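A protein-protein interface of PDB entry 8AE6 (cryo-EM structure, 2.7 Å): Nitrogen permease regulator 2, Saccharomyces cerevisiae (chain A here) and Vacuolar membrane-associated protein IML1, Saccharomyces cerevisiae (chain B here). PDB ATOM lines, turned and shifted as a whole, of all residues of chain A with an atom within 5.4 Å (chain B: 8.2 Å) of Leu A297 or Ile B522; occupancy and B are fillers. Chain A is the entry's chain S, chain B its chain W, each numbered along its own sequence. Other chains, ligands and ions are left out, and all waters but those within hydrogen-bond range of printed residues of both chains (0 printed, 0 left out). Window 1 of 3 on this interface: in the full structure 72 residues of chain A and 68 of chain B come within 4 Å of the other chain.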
ATOM      1  N   LEU A 251      17.703 -26.035 -16.876  1.00  0.00           N
ATOM      2  CA  LEU A 251      18.391 -25.344 -15.797  1.00  0.00           C
ATOM      3  C   LEU A 251      19.780 -24.851 -16.174  1.00  0.00           C
ATOM      4  O   LEU A 251      20.361 -24.067 -15.416  1.00  0.00           O
ATOM      5  CB  LEU A 251      18.493 -26.254 -14.571  1.00  0.00           C
ATOM      6  CG  LEU A 251      17.201 -26.546 -13.811  1.00  0.00           C
ATOM      7  CD1 LEU A 251      17.445 -27.595 -12.745  1.00  0.00           C
ATOM      8  CD2 LEU A 251      16.649 -25.278 -13.192  1.00  0.00           C
ATOM      9  N   ILE A 254      19.464 -21.006 -17.216  1.00  0.00           N
ATOM     10  CA  ILE A 254      19.076 -20.075 -16.160  1.00  0.00           C
ATOM     11  C   ILE A 254      20.252 -19.694 -15.276  1.00  0.00           C
ATOM     12  O   ILE A 254      20.177 -18.688 -14.559  1.00  0.00           O
ATOM     13  CB  ILE A 254      17.931 -20.697 -15.337  1.00  0.00           C
ATOM     14  CG1 ILE A 254      16.948 -21.407 -16.259  1.00  0.00           C
ATOM     15  CG2 ILE A 254      17.154 -19.650 -14.557  1.00  0.00           C
ATOM     16  CD1 ILE A 254      15.822 -22.087 -15.526  1.00  0.00           C
ATOM     17  N   TRP A 259      23.932 -17.355  -8.783  1.00  0.00           N
ATOM     18  CA  TRP A 259      23.417 -18.594  -8.221  1.00  0.00           C
ATOM     19  C   TRP A 259      24.308 -19.080  -7.083  1.00  0.00           C
ATOM     20  O   TRP A 259      25.496 -18.754  -7.000  1.00  0.00           O
ATOM     21  CB  TRP A 259      23.314 -19.675  -9.295  1.00  0.00           C
ATOM     22  CG  TRP A 259      22.020 -19.671 -10.023  1.00  0.00           C
ATOM     23  CD1 TRP A 259      21.306 -18.584 -10.402  1.00  0.00           C
ATOM     24  CD2 TRP A 259      21.280 -20.809 -10.465  1.00  0.00           C
ATOM     25  NE1 TRP A 259      20.167 -18.966 -11.059  1.00  0.00           N
ATOM     26  CE2 TRP A 259      20.127 -20.333 -11.109  1.00  0.00           C
ATOM     27  CE3 TRP A 259      21.482 -22.187 -10.379  1.00  0.00           C
ATOM     28  CZ2 TRP A 259      19.177 -21.181 -11.663  1.00  0.00           C
ATOM     29  CZ3 TRP A 259      20.539 -23.023 -10.926  1.00  0.00           C
ATOM     30  CH2 TRP A 259      19.403 -22.522 -11.560  1.00  0.00           C
ATOM     31  N   MET A 263      23.715 -25.084  -5.662  1.00  0.00           N
ATOM     32  CA  MET A 263      22.714 -25.286  -6.707  1.00  0.00           C
ATOM     33  C   MET A 263      23.356 -25.451  -8.078  1.00  0.00           C
ATOM     34  O   MET A 263      22.907 -26.275  -8.891  1.00  0.00           O
ATOM     35  CB  MET A 263      21.734 -24.117  -6.725  1.00  0.00           C
ATOM     36  CG  MET A 263      20.348 -24.476  -7.212  1.00  0.00           C
ATOM     37  SD  MET A 263      19.194 -23.105  -7.059  1.00  0.00           S
ATOM     38  CE  MET A 263      18.754 -23.234  -5.333  1.00  0.00           C
ATOM     39  N   ILE A 270      20.423 -33.361 -12.148  1.00  0.00           N
ATOM     40  CA  ILE A 270      18.964 -33.541 -12.066  1.00  0.00           C
ATOM     41  C   ILE A 270      18.527 -34.026 -13.442  1.00  0.00           C
ATOM     42  O   ILE A 270      18.098 -33.264 -14.311  1.00  0.00           O
ATOM     43  CB  ILE A 270      18.247 -32.261 -11.628  1.00  0.00           C
ATOM     44  CG1 ILE A 270      18.879 -31.702 -10.357  1.00  0.00           C
ATOM     45  CG2 ILE A 270      16.770 -32.529 -11.397  1.00  0.00           C
ATOM     46  CD1 ILE A 270      18.214 -30.452  -9.850  1.00  0.00           C
ATOM     47  N   GLU A 292      17.650 -28.129   0.765  1.00  0.00           N
ATOM     48  CA  GLU A 292      17.271 -26.719   0.723  1.00  0.00           C
ATOM     49  C   GLU A 292      17.319 -26.149  -0.693  1.00  0.00           C
ATOM     50  O   GLU A 292      16.482 -25.309  -1.044  1.00  0.00           O
ATOM     51  CB  GLU A 292      18.165 -25.911   1.657  1.00  0.00           C
ATOM     52  CG  GLU A 292      17.807 -26.064   3.122  1.00  0.00           C
ATOM     53  CD  GLU A 292      16.921 -24.942   3.623  1.00  0.00           C
ATOM     54  OE1 GLU A 292      16.403 -24.175   2.786  1.00  0.00           O
ATOM     55  OE2 GLU A 292      16.743 -24.829   4.854  1.00  0.00           O
ATOM     56  N   CYS A 293      18.268 -26.592  -1.522  1.00  0.00           N
ATOM     57  CA  CYS A 293      18.329 -26.115  -2.903  1.00  0.00           C
ATOM     58  C   CYS A 293      17.167 -26.655  -3.730  1.00  0.00           C
ATOM     59  O   CYS A 293      16.599 -25.931  -4.559  1.00  0.00           O
ATOM     60  CB  CYS A 293      19.663 -26.500  -3.535  1.00  0.00           C
ATOM     61  SG  CYS A 293      21.071 -25.550  -2.925  1.00  0.00           S
ATOM     62  N   ILE A 294      16.793 -27.917  -3.510  1.00  0.00           N
ATOM     63  CA  ILE A 294      15.615 -28.477  -4.165  1.00  0.00           C
ATOM     64  C   ILE A 294      14.359 -27.758  -3.687  1.00  0.00           C
ATOM     65  O   ILE A 294      13.435 -27.509  -4.468  1.00  0.00           O
ATOM     66  CB  ILE A 294      15.550 -29.998  -3.923  1.00  0.00           C
ATOM     67  CG1 ILE A 294      16.669 -30.707  -4.685  1.00  0.00           C
ATOM     68  CG2 ILE A 294      14.216 -30.589  -4.353  1.00  0.00           C
ATOM     69  CD1 ILE A 294      16.607 -30.514  -6.182  1.00  0.00           C
ATOM     70  N   ARG A 295      14.326 -27.368  -2.408  1.00  0.00           N
ATOM     71  CA  ARG A 295      13.207 -26.589  -1.884  1.00  0.00           C
ATOM     72  C   ARG A 295      13.123 -25.217  -2.543  1.00  0.00           C
ATOM     73  O   ARG A 295      12.028 -24.744  -2.869  1.00  0.00           O
ATOM     74  CB  ARG A 295      13.344 -26.446  -0.371  1.00  0.00           C
ATOM     75  CG  ARG A 295      12.726 -27.578   0.418  1.00  0.00           C
ATOM     76  CD  ARG A 295      12.886 -27.350   1.903  1.00  0.00           C
ATOM     77  NE  ARG A 295      11.728 -26.673   2.467  1.00  0.00           N
ATOM     78  CZ  ARG A 295      11.789 -25.774   3.437  1.00  0.00           C
ATOM     79  NH1 ARG A 295      12.943 -25.418   3.978  1.00  0.00           N
ATOM     80  NH2 ARG A 295      10.667 -25.214   3.877  1.00  0.00           N
ATOM     81  N   HIS A 296      14.269 -24.564  -2.748  1.00  0.00           N
ATOM     82  CA  HIS A 296      14.281 -23.268  -3.419  1.00  0.00           C
ATOM     83  C   HIS A 296      13.842 -23.392  -4.870  1.00  0.00           C
ATOM     84  O   HIS A 296      13.150 -22.512  -5.393  1.00  0.00           O
ATOM     85  CB  HIS A 296      15.672 -22.643  -3.338  1.00  0.00           C
ATOM     86  CG  HIS A 296      16.024 -22.121  -1.981  1.00  0.00           C
ATOM     87  ND1 HIS A 296      16.729 -22.866  -1.059  1.00  0.00           N
ATOM     88  CD2 HIS A 296      15.778 -20.929  -1.394  1.00  0.00           C
ATOM     89  CE1 HIS A 296      16.896 -22.155   0.041  1.00  0.00           C
ATOM     90  NE2 HIS A 296      16.327 -20.977  -0.137  1.00  0.00           N
ATOM     91  N   LEU A 297      14.230 -24.479  -5.540  1.00  0.00           N
ATOM     92  CA  LEU A 297      13.780 -24.700  -6.910  1.00  0.00           C
ATOM     93  C   LEU A 297      12.301 -25.064  -6.971  1.00  0.00           C
ATOM     94  O   LEU A 297      11.633 -24.776  -7.969  1.00  0.00           O
ATOM     95  CB  LEU A 297      14.630 -25.781  -7.567  1.00  0.00           C
ATOM     96  CG  LEU A 297      16.010 -25.346  -8.055  1.00  0.00           C
ATOM     97  CD1 LEU A 297      16.899 -26.553  -8.271  1.00  0.00           C
ATOM     98  CD2 LEU A 297      15.891 -24.539  -9.331  1.00  0.00           C
ATOM     99  N   ILE A 298      11.781 -25.707  -5.924  1.00  0.00           N
ATOM    100  CA  ILE A 298      10.344 -25.948  -5.808  1.00  0.00           C
ATOM    101  C   ILE A 298       9.603 -24.628  -5.642  1.00  0.00           C
ATOM    102  O   ILE A 298       8.528 -24.422  -6.221  1.00  0.00           O
ATOM    103  CB  ILE A 298      10.073 -26.918  -4.639  1.00  0.00           C
ATOM    104  CG1 ILE A 298      10.344 -28.360  -5.063  1.00  0.00           C
ATOM    105  CG2 ILE A 298       8.650 -26.803  -4.108  1.00  0.00           C
ATOM    106  CD1 ILE A 298      10.651 -29.281  -3.911  1.00  0.00           C
ATOM    107  N   TYR A 299      10.192 -23.702  -4.877  1.00  0.00           N
ATOM    108  CA  TYR A 299       9.591 -22.394  -4.626  1.00  0.00           C
ATOM    109  C   TYR A 299       9.422 -21.583  -5.904  1.00  0.00           C
ATOM    110  O   TYR A 299       8.500 -20.765  -6.001  1.00  0.00           O
ATOM    111  CB  TYR A 299      10.452 -21.638  -3.615  1.00  0.00           C
ATOM    112  CG  TYR A 299      10.038 -20.212  -3.356  1.00  0.00           C
ATOM    113  CD1 TYR A 299       8.889 -19.922  -2.639  1.00  0.00           C
ATOM    114  CD2 TYR A 299      10.812 -19.153  -3.812  1.00  0.00           C
ATOM    115  CE1 TYR A 299       8.514 -18.621  -2.388  1.00  0.00           C
ATOM    116  CE2 TYR A 299      10.444 -17.849  -3.571  1.00  0.00           C
ATOM    117  CZ  TYR A 299       9.294 -17.588  -2.861  1.00  0.00           C
ATOM    118  OH  TYR A 299       8.922 -16.287  -2.617  1.00  0.00           O
ATOM    119  N   TYR A 300      10.282 -21.800  -6.896  1.00  0.00           N
ATOM    120  CA  TYR A 300      10.181 -21.121  -8.178  1.00  0.00           C
ATOM    121  C   TYR A 300       9.437 -21.940  -9.223  1.00  0.00           C
ATOM    122  O   TYR A 300       9.452 -21.570 -10.402  1.00  0.00           O
ATOM    123  CB  TYR A 300      11.575 -20.756  -8.688  1.00  0.00           C
ATOM    124  CG  TYR A 300      12.214 -19.629  -7.913  1.00  0.00           C
ATOM    125  CD1 TYR A 300      11.692 -18.345  -7.967  1.00  0.00           C
ATOM    126  CD2 TYR A 300      13.327 -19.851  -7.121  1.00  0.00           C
ATOM    127  CE1 TYR A 300      12.269 -17.314  -7.258  1.00  0.00           C
ATOM    128  CE2 TYR A 300      13.910 -18.829  -6.407  1.00  0.00           C
ATOM    129  CZ  TYR A 300      13.379 -17.562  -6.479  1.00  0.00           C
ATOM    130  OH  TYR A 300      13.959 -16.538  -5.769  1.00  0.00           O
ATOM    131  N   LYS A 301       8.803 -23.047  -8.809  1.00  0.00           N
ATOM    132  CA  LYS A 301       7.933 -23.875  -9.652  1.00  0.00           C
ATOM    133  C   LYS A 301       8.675 -24.437 -10.862  1.00  0.00           C
ATOM    134  O   LYS A 301       8.267 -24.258 -12.011  1.00  0.00           O
ATOM    135  CB  LYS A 301       6.683 -23.104 -10.085  1.00  0.00           C
ATOM    136  CG  LYS A 301       5.844 -22.574  -8.940  1.00  0.00           C
ATOM    137  CD  LYS A 301       5.196 -23.709  -8.171  1.00  0.00           C
ATOM    138  CE  LYS A 301       4.154 -24.422  -9.018  1.00  0.00           C
ATOM    139  NZ  LYS A 301       2.994 -23.544  -9.334  1.00  0.00           N
ATOM    140  N   CYS A 302       9.782 -25.126 -10.597  1.00  0.00           N
ATOM    141  CA  CYS A 302      10.599 -25.680 -11.665  1.00  0.00           C
ATOM    142  C   CYS A 302      11.075 -27.102 -11.425  1.00  0.00           C
ATOM    143  O   CYS A 302      11.582 -27.724 -12.365  1.00  0.00           O
ATOM    144  CB  CYS A 302      11.813 -24.781 -11.919  1.00  0.00           C
ATOM    145  SG  CYS A 302      11.361 -23.265 -12.786  1.00  0.00           S
ATOM    146  N   VAL A 303      10.941 -27.634 -10.213  1.00  0.00           N
ATOM    147  CA  VAL A 303      11.334 -28.999  -9.892  1.00  0.00           C
ATOM    148  C   VAL A 303      10.183 -29.694  -9.178  1.00  0.00           C
ATOM    149  O   VAL A 303       9.656 -29.176  -8.189  1.00  0.00           O
ATOM    150  CB  VAL A 303      12.611 -29.039  -9.030  1.00  0.00           C
ATOM    151  CG1 VAL A 303      12.906 -30.439  -8.629  1.00  0.00           C
ATOM    152  CG2 VAL A 303      13.792 -28.520  -9.819  1.00  0.00           C
ATOM    153  N   PHE B 292      16.299  -6.404  -7.791  1.00  0.00           N
ATOM    154  CA  PHE B 292      15.220  -6.435  -6.819  1.00  0.00           C
ATOM    155  C   PHE B 292      15.351  -7.636  -5.894  1.00  0.00           C
ATOM    156  O   PHE B 292      15.697  -8.739  -6.323  1.00  0.00           O
ATOM    157  CB  PHE B 292      13.874  -6.484  -7.529  1.00  0.00           C
ATOM    158  CG  PHE B 292      13.402  -5.155  -8.011  1.00  0.00           C
ATOM    159  CD1 PHE B 292      12.712  -4.304  -7.165  1.00  0.00           C
ATOM    160  CD2 PHE B 292      13.637  -4.757  -9.312  1.00  0.00           C
ATOM    161  CE1 PHE B 292      12.272  -3.076  -7.609  1.00  0.00           C
ATOM    162  CE2 PHE B 292      13.201  -3.535  -9.762  1.00  0.00           C
ATOM    163  CZ  PHE B 292      12.518  -2.692  -8.910  1.00  0.00           C
ATOM    164  N   GLU B 294      13.506 -10.352  -3.157  1.00  0.00           N
ATOM    165  CA  GLU B 294      12.278 -11.136  -3.267  1.00  0.00           C
ATOM    166  C   GLU B 294      11.080 -10.413  -2.665  1.00  0.00           C
ATOM    167  O   GLU B 294       9.943 -10.638  -3.093  1.00  0.00           O
ATOM    168  CB  GLU B 294      12.462 -12.489  -2.582  1.00  0.00           C
ATOM    169  CG  GLU B 294      13.416 -13.431  -3.286  1.00  0.00           C
ATOM    170  CD  GLU B 294      14.791 -13.426  -2.653  1.00  0.00           C
ATOM    171  OE1 GLU B 294      15.053 -12.540  -1.812  1.00  0.00           O
ATOM    172  OE2 GLU B 294      15.608 -14.312  -2.984  1.00  0.00           O
ATOM    173  N   TRP B 516       9.516 -19.248   6.283  1.00  0.00           N
ATOM    174  CA  TRP B 516      10.525 -19.574   5.288  1.00  0.00           C
ATOM    175  C   TRP B 516      10.928 -18.337   4.496  1.00  0.00           C
ATOM    176  O   TRP B 516      10.077 -17.553   4.065  1.00  0.00           O
ATOM    177  CB  TRP B 516      10.008 -20.651   4.337  1.00  0.00           C
ATOM    178  CG  TRP B 516      11.074 -21.234   3.473  1.00  0.00           C
ATOM    179  CD1 TRP B 516      11.998 -22.171   3.831  1.00  0.00           C
ATOM    180  CD2 TRP B 516      11.336 -20.914   2.105  1.00  0.00           C
ATOM    181  NE1 TRP B 516      12.816 -22.458   2.766  1.00  0.00           N
ATOM    182  CE2 TRP B 516      12.431 -21.698   1.695  1.00  0.00           C
ATOM    183  CE3 TRP B 516      10.753 -20.038   1.187  1.00  0.00           C
ATOM    184  CZ2 TRP B 516      12.950 -21.636   0.411  1.00  0.00           C
ATOM    185  CZ3 TRP B 516      11.271 -19.978  -0.088  1.00  0.00           C
ATOM    186  CH2 TRP B 516      12.357 -20.772  -0.467  1.00  0.00           C
ATOM    187  N   PRO B 518      13.469 -17.139   1.173  1.00  0.00           N
ATOM    188  CA  PRO B 518      14.313 -17.618   0.067  1.00  0.00           C
ATOM    189  C   PRO B 518      15.740 -17.108   0.166  1.00  0.00           C
ATOM    190  O   PRO B 518      16.002 -15.922  -0.055  1.00  0.00           O
ATOM    191  CB  PRO B 518      13.609 -17.066  -1.180  1.00  0.00           C
ATOM    192  CG  PRO B 518      12.266 -16.599  -0.723  1.00  0.00           C
ATOM    193  CD  PRO B 518      12.406 -16.237   0.712  1.00  0.00           C
ATOM    194  N   ARG B 519      16.669 -18.001   0.493  1.00  0.00           N
ATOM    195  CA  ARG B 519      18.063 -17.642   0.705  1.00  0.00           C
ATOM    196  C   ARG B 519      18.950 -17.924  -0.499  1.00  0.00           C
ATOM    197  O   ARG B 519      20.155 -17.669  -0.435  1.00  0.00           O
ATOM    198  CB  ARG B 519      18.607 -18.380   1.930  1.00  0.00           C
ATOM    199  CG  ARG B 519      17.801 -18.143   3.188  1.00  0.00           C
ATOM    200  CD  ARG B 519      18.580 -18.522   4.433  1.00  0.00           C
ATOM    201  NE  ARG B 519      17.873 -18.147   5.652  1.00  0.00           N
ATOM    202  CZ  ARG B 519      17.858 -16.926   6.169  1.00  0.00           C
ATOM    203  NH1 ARG B 519      18.512 -15.926   5.599  1.00  0.00           N
ATOM    204  NH2 ARG B 519      17.172 -16.701   7.285  1.00  0.00           N
ATOM    205  N   CYS B 520      18.391 -18.440  -1.590  1.00  0.00           N
ATOM    206  CA  CYS B 520      19.127 -18.676  -2.824  1.00  0.00           C
ATOM    207  C   CYS B 520      18.528 -17.819  -3.929  1.00  0.00           C
ATOM    208  O   CYS B 520      17.307 -17.774  -4.099  1.00  0.00           O
ATOM    209  CB  CYS B 520      19.087 -20.151  -3.224  1.00  0.00           C
ATOM    210  SG  CYS B 520      20.230 -21.204  -2.310  1.00  0.00           S
ATOM    211  N   LYS B 521      19.392 -17.142  -4.678  1.00  0.00           N
ATOM    212  CA  LYS B 521      18.972 -16.150  -5.662  1.00  0.00           C
ATOM    213  C   LYS B 521      18.926 -16.792  -7.042  1.00  0.00           C
ATOM    214  O   LYS B 521      19.953 -17.241  -7.560  1.00  0.00           O
ATOM    215  CB  LYS B 521      19.921 -14.954  -5.655  1.00  0.00           C
ATOM    216  CG  LYS B 521      19.432 -13.770  -4.845  1.00  0.00           C
ATOM    217  CD  LYS B 521      20.453 -12.649  -4.852  1.00  0.00           C
ATOM    218  CE  LYS B 521      19.853 -11.353  -4.333  1.00  0.00           C
ATOM    219  NZ  LYS B 521      18.701 -10.904  -5.161  1.00  0.00           N
ATOM    220  N   ILE B 522      17.739 -16.837  -7.632  1.00  0.00           N
ATOM    221  CA  ILE B 522      17.555 -17.207  -9.030  1.00  0.00           C
ATOM    222  C   ILE B 522      16.903 -16.009  -9.701  1.00  0.00           C
ATOM    223  O   ILE B 522      15.692 -15.797  -9.574  1.00  0.00           O
ATOM    224  CB  ILE B 522      16.710 -18.471  -9.202  1.00  0.00           C
ATOM    225  CG1 ILE B 522      17.320 -19.633  -8.421  1.00  0.00           C
ATOM    226  CG2 ILE B 522      16.607 -18.822 -10.665  1.00  0.00           C
ATOM    227  CD1 ILE B 522      16.539 -20.915  -8.533  1.00  0.00           C
ATOM    228  N   TYR B 523      17.700 -15.215 -10.413  1.00  0.00           N
ATOM    229  CA  TYR B 523      17.218 -13.937 -10.924  1.00  0.00           C
ATOM    230  C   TYR B 523      16.305 -14.109 -12.129  1.00  0.00           C
ATOM    231  O   TYR B 523      15.333 -13.363 -12.282  1.00  0.00           O
ATOM    232  CB  TYR B 523      18.400 -13.039 -11.282  1.00  0.00           C
ATOM    233  CG  TYR B 523      18.059 -11.570 -11.324  1.00  0.00           C
ATOM    234  CD1 TYR B 523      17.781 -10.870 -10.157  1.00  0.00           C
ATOM    235  CD2 TYR B 523      18.017 -10.881 -12.529  1.00  0.00           C
ATOM    236  CE1 TYR B 523      17.467  -9.526 -10.187  1.00  0.00           C
ATOM    237  CE2 TYR B 523      17.704  -9.534 -12.572  1.00  0.00           C
ATOM    238  CZ  TYR B 523      17.431  -8.862 -11.396  1.00  0.00           C
ATOM    239  OH  TYR B 523      17.119  -7.524 -11.432  1.00  0.00           O
ATOM    240  N   ASP B 524      16.597 -15.081 -12.993  1.00  0.00           N
ATOM    241  CA  ASP B 524      15.831 -15.231 -14.222  1.00  0.00           C
ATOM    242  C   ASP B 524      14.454 -15.831 -13.985  1.00  0.00           C
ATOM    243  O   ASP B 524      13.579 -15.700 -14.848  1.00  0.00           O
ATOM    244  CB  ASP B 524      16.610 -16.089 -15.218  1.00  0.00           C
ATOM    245  CG  ASP B 524      17.822 -15.374 -15.775  1.00  0.00           C
ATOM    246  OD1 ASP B 524      18.119 -14.254 -15.312  1.00  0.00           O
ATOM    247  OD2 ASP B 524      18.477 -15.935 -16.675  1.00  0.00           O
ATOM    248  N   LEU B 525      14.236 -16.484 -12.846  1.00  0.00           N
ATOM    249  CA  LEU B 525      12.921 -17.004 -12.505  1.00  0.00           C
ATOM    250  C   LEU B 525      12.134 -16.079 -11.592  1.00  0.00           C
ATOM    251  O   LEU B 525      10.902 -16.068 -11.657  1.00  0.00           O
ATOM    252  CB  LEU B 525      13.049 -18.378 -11.838  1.00  0.00           C
ATOM    253  CG  LEU B 525      13.408 -19.520 -12.785  1.00  0.00           C
ATOM    254  CD1 LEU B 525      13.804 -20.751 -12.003  1.00  0.00           C
ATOM    255  CD2 LEU B 525      12.249 -19.819 -13.718  1.00  0.00           C
ATOM    256  N   GLN B 526      12.816 -15.316 -10.739  1.00  0.00           N
ATOM    257  CA  GLN B 526      12.135 -14.300  -9.946  1.00  0.00           C
ATOM    258  C   GLN B 526      11.641 -13.159 -10.823  1.00  0.00           C
ATOM    259  O   GLN B 526      10.496 -12.714 -10.690  1.00  0.00           O
ATOM    260  CB  GLN B 526      13.071 -13.782  -8.854  1.00  0.00           C
ATOM    261  CG  GLN B 526      12.670 -12.448  -8.260  1.00  0.00           C
ATOM    262  CD  GLN B 526      13.765 -11.836  -7.419  1.00  0.00           C
ATOM    263  OE1 GLN B 526      14.753 -12.494  -7.098  1.00  0.00           O
ATOM    264  NE2 GLN B 526      13.600 -10.570  -7.060  1.00  0.00           N
ATOM    265  N   MET B 527      12.485 -12.686 -11.741  1.00  0.00           N
ATOM    266  CA  MET B 527      12.109 -11.615 -12.653  1.00  0.00           C
ATOM    267  C   MET B 527      11.354 -12.112 -13.875  1.00  0.00           C
ATOM    268  O   MET B 527      10.892 -11.279 -14.663  1.00  0.00           O
ATOM    269  CB  MET B 527      13.350 -10.847 -13.109  1.00  0.00           C
ATOM    270  CG  MET B 527      14.154 -10.231 -11.981  1.00  0.00           C
ATOM    271  SD  MET B 527      13.317  -8.845 -11.199  1.00  0.00           S
ATOM    272  CE  MET B 527      13.847  -7.497 -12.244  1.00  0.00           C
ATOM    273  N   MET B 528      11.216 -13.433 -14.029  1.00  0.00           N
ATOM    274  CA  MET B 528      10.611 -14.074 -15.202  1.00  0.00           C
ATOM    275  C   MET B 528      11.281 -13.612 -16.494  1.00  0.00           C
ATOM    276  O   MET B 528      10.622 -13.295 -17.486  1.00  0.00           O
ATOM    277  CB  MET B 528       9.098 -13.842 -15.247  1.00  0.00           C
ATOM    278  CG  MET B 528       8.323 -14.657 -14.230  1.00  0.00           C
ATOM    279  SD  MET B 528       6.622 -14.962 -14.732  1.00  0.00           S
ATOM    280  CE  MET B 528       5.992 -15.823 -13.294  1.00  0.00           C
ATOM    281  N   GLY B 529      12.614 -13.572 -16.473  1.00  0.00           N
ATOM    282  CA  GLY B 529      13.369 -13.059 -17.601  1.00  0.00           C
ATOM    283  C   GLY B 529      13.458 -13.991 -18.784  1.00  0.00           C
ATOM    284  O   GLY B 529      13.857 -13.557 -19.871  1.00  0.00           O
ATOM    285  N   ILE B 530      13.103 -15.258 -18.607  1.00  0.00           N
ATOM    286  CA  ILE B 530      13.156 -16.243 -19.681  1.00  0.00           C
ATOM    287  C   ILE B 530      11.728 -16.559 -20.106  1.00  0.00           C
ATOM    288  O   ILE B 530      10.893 -16.941 -19.277  1.00  0.00           O
ATOM    289  CB  ILE B 530      13.904 -17.511 -19.244  1.00  0.00           C
ATOM    290  CG1 ILE B 530      15.169 -17.141 -18.470  1.00  0.00           C
ATOM    291  CG2 ILE B 530      14.267 -18.349 -20.449  1.00  0.00           C
ATOM    292  CD1 ILE B 530      16.228 -16.446 -19.308  1.00  0.00           C
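The backbone carbonyl oxygen (O) of Phe B292 sits at hydrogen-bond distance from the side-chain amide nitrogen (NE2) of Gln B526, at 2.9 Å. A ring nitrogen (ND1) of His A296 is in hydrogen-bond range of the backbone carbonyl oxygen (O) of Glu A292, 2.5 Å away. O of Asp B524 is in hydrogen-bond range of N of Gly B529 (2.8 Å). The guanidinium group of Arg A295 lies within salt-bridge range of the side-chain carboxylate of Glu A292 (3.9 Å). The backbone NH (N) of Cys A302 lies within hydrogen-bond range of the backbone carbonyl oxygen (O) of Leu A297, 3.2 Å away. The side-chain sulfur of Cys A302 lies within hydrogen-bond range of the backbone carbonyl oxygen of Tyr A300 (3.5 Å).
Of the 17 printed residues of chain A, 10 touch a printed residue of chain B. Printed residues of chain A that touch a printed residue of chain B: Ile A254, Trp A259, Met A263, Glu A292, Arg A295, His A296, Leu A297, Tyr A299, Tyr A300 and Cys A302. Hydrophobic or aromatic side chains of chain A that line the printed part of chain B: Ile A254, Trp A259, Met A263, His A296, Leu A297, Tyr A299 and Tyr A300. Of the 16 printed residues of chain B, 10 touch a printed residue of chain A. Along chain B the printed residues that touch a printed residue of chain A span positions 294 to 526.
CB of Cys B520 touches CE of Met A263, 3.8 Å away. Met A263 touches Ile B522. Trp B516 touches Glu A292. Trp B516 touches His A296. NE2 of His A296 touches N of Cys B520 (3.6 Å). CD2 of Leu A297 touches CD1 of Ile B522 (3.8 Å). Trp B516 touches Tyr A299. OE2 of Glu B294 touches OH of Tyr A300 (3.9 Å). CE1 of Tyr A300 touches CB of Gln B526 (3.96 Å). CD1 of Leu B525 touches SG of Cys A302, at 3.6 Å.
Of the printed residues of chain B, Met A263 touches Cys B520 and Ile B522. Leu A297 touches just one residue of chain B: Ile B522. Of the printed residues of chain A, Pro B518 touches His A296 (3.9 Å) and Tyr A299 (3.6 Å). Printed residues of chain A within 4 Å of Ile B522: Trp A259 (3.6 Å), Met A263 (3.7 Å), Leu A297 (3.8 Å) and Tyr A300 (3.7 Å). The nearest printed residue of chain A that does not touch Ile B522 is Ile A254 (4.02 Å). The nearest printed residue of chain A that does not touch Arg B519 is Glu A292 (6.2 Å).
The guanidinium group (NH1) of Arg A295 sits close to the indole nitrogen (NE1) of Trp B516 (3.2 Å). NE2 of His A296 is in hydrogen-bond range of N of Arg B519, 3.1 Å away.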
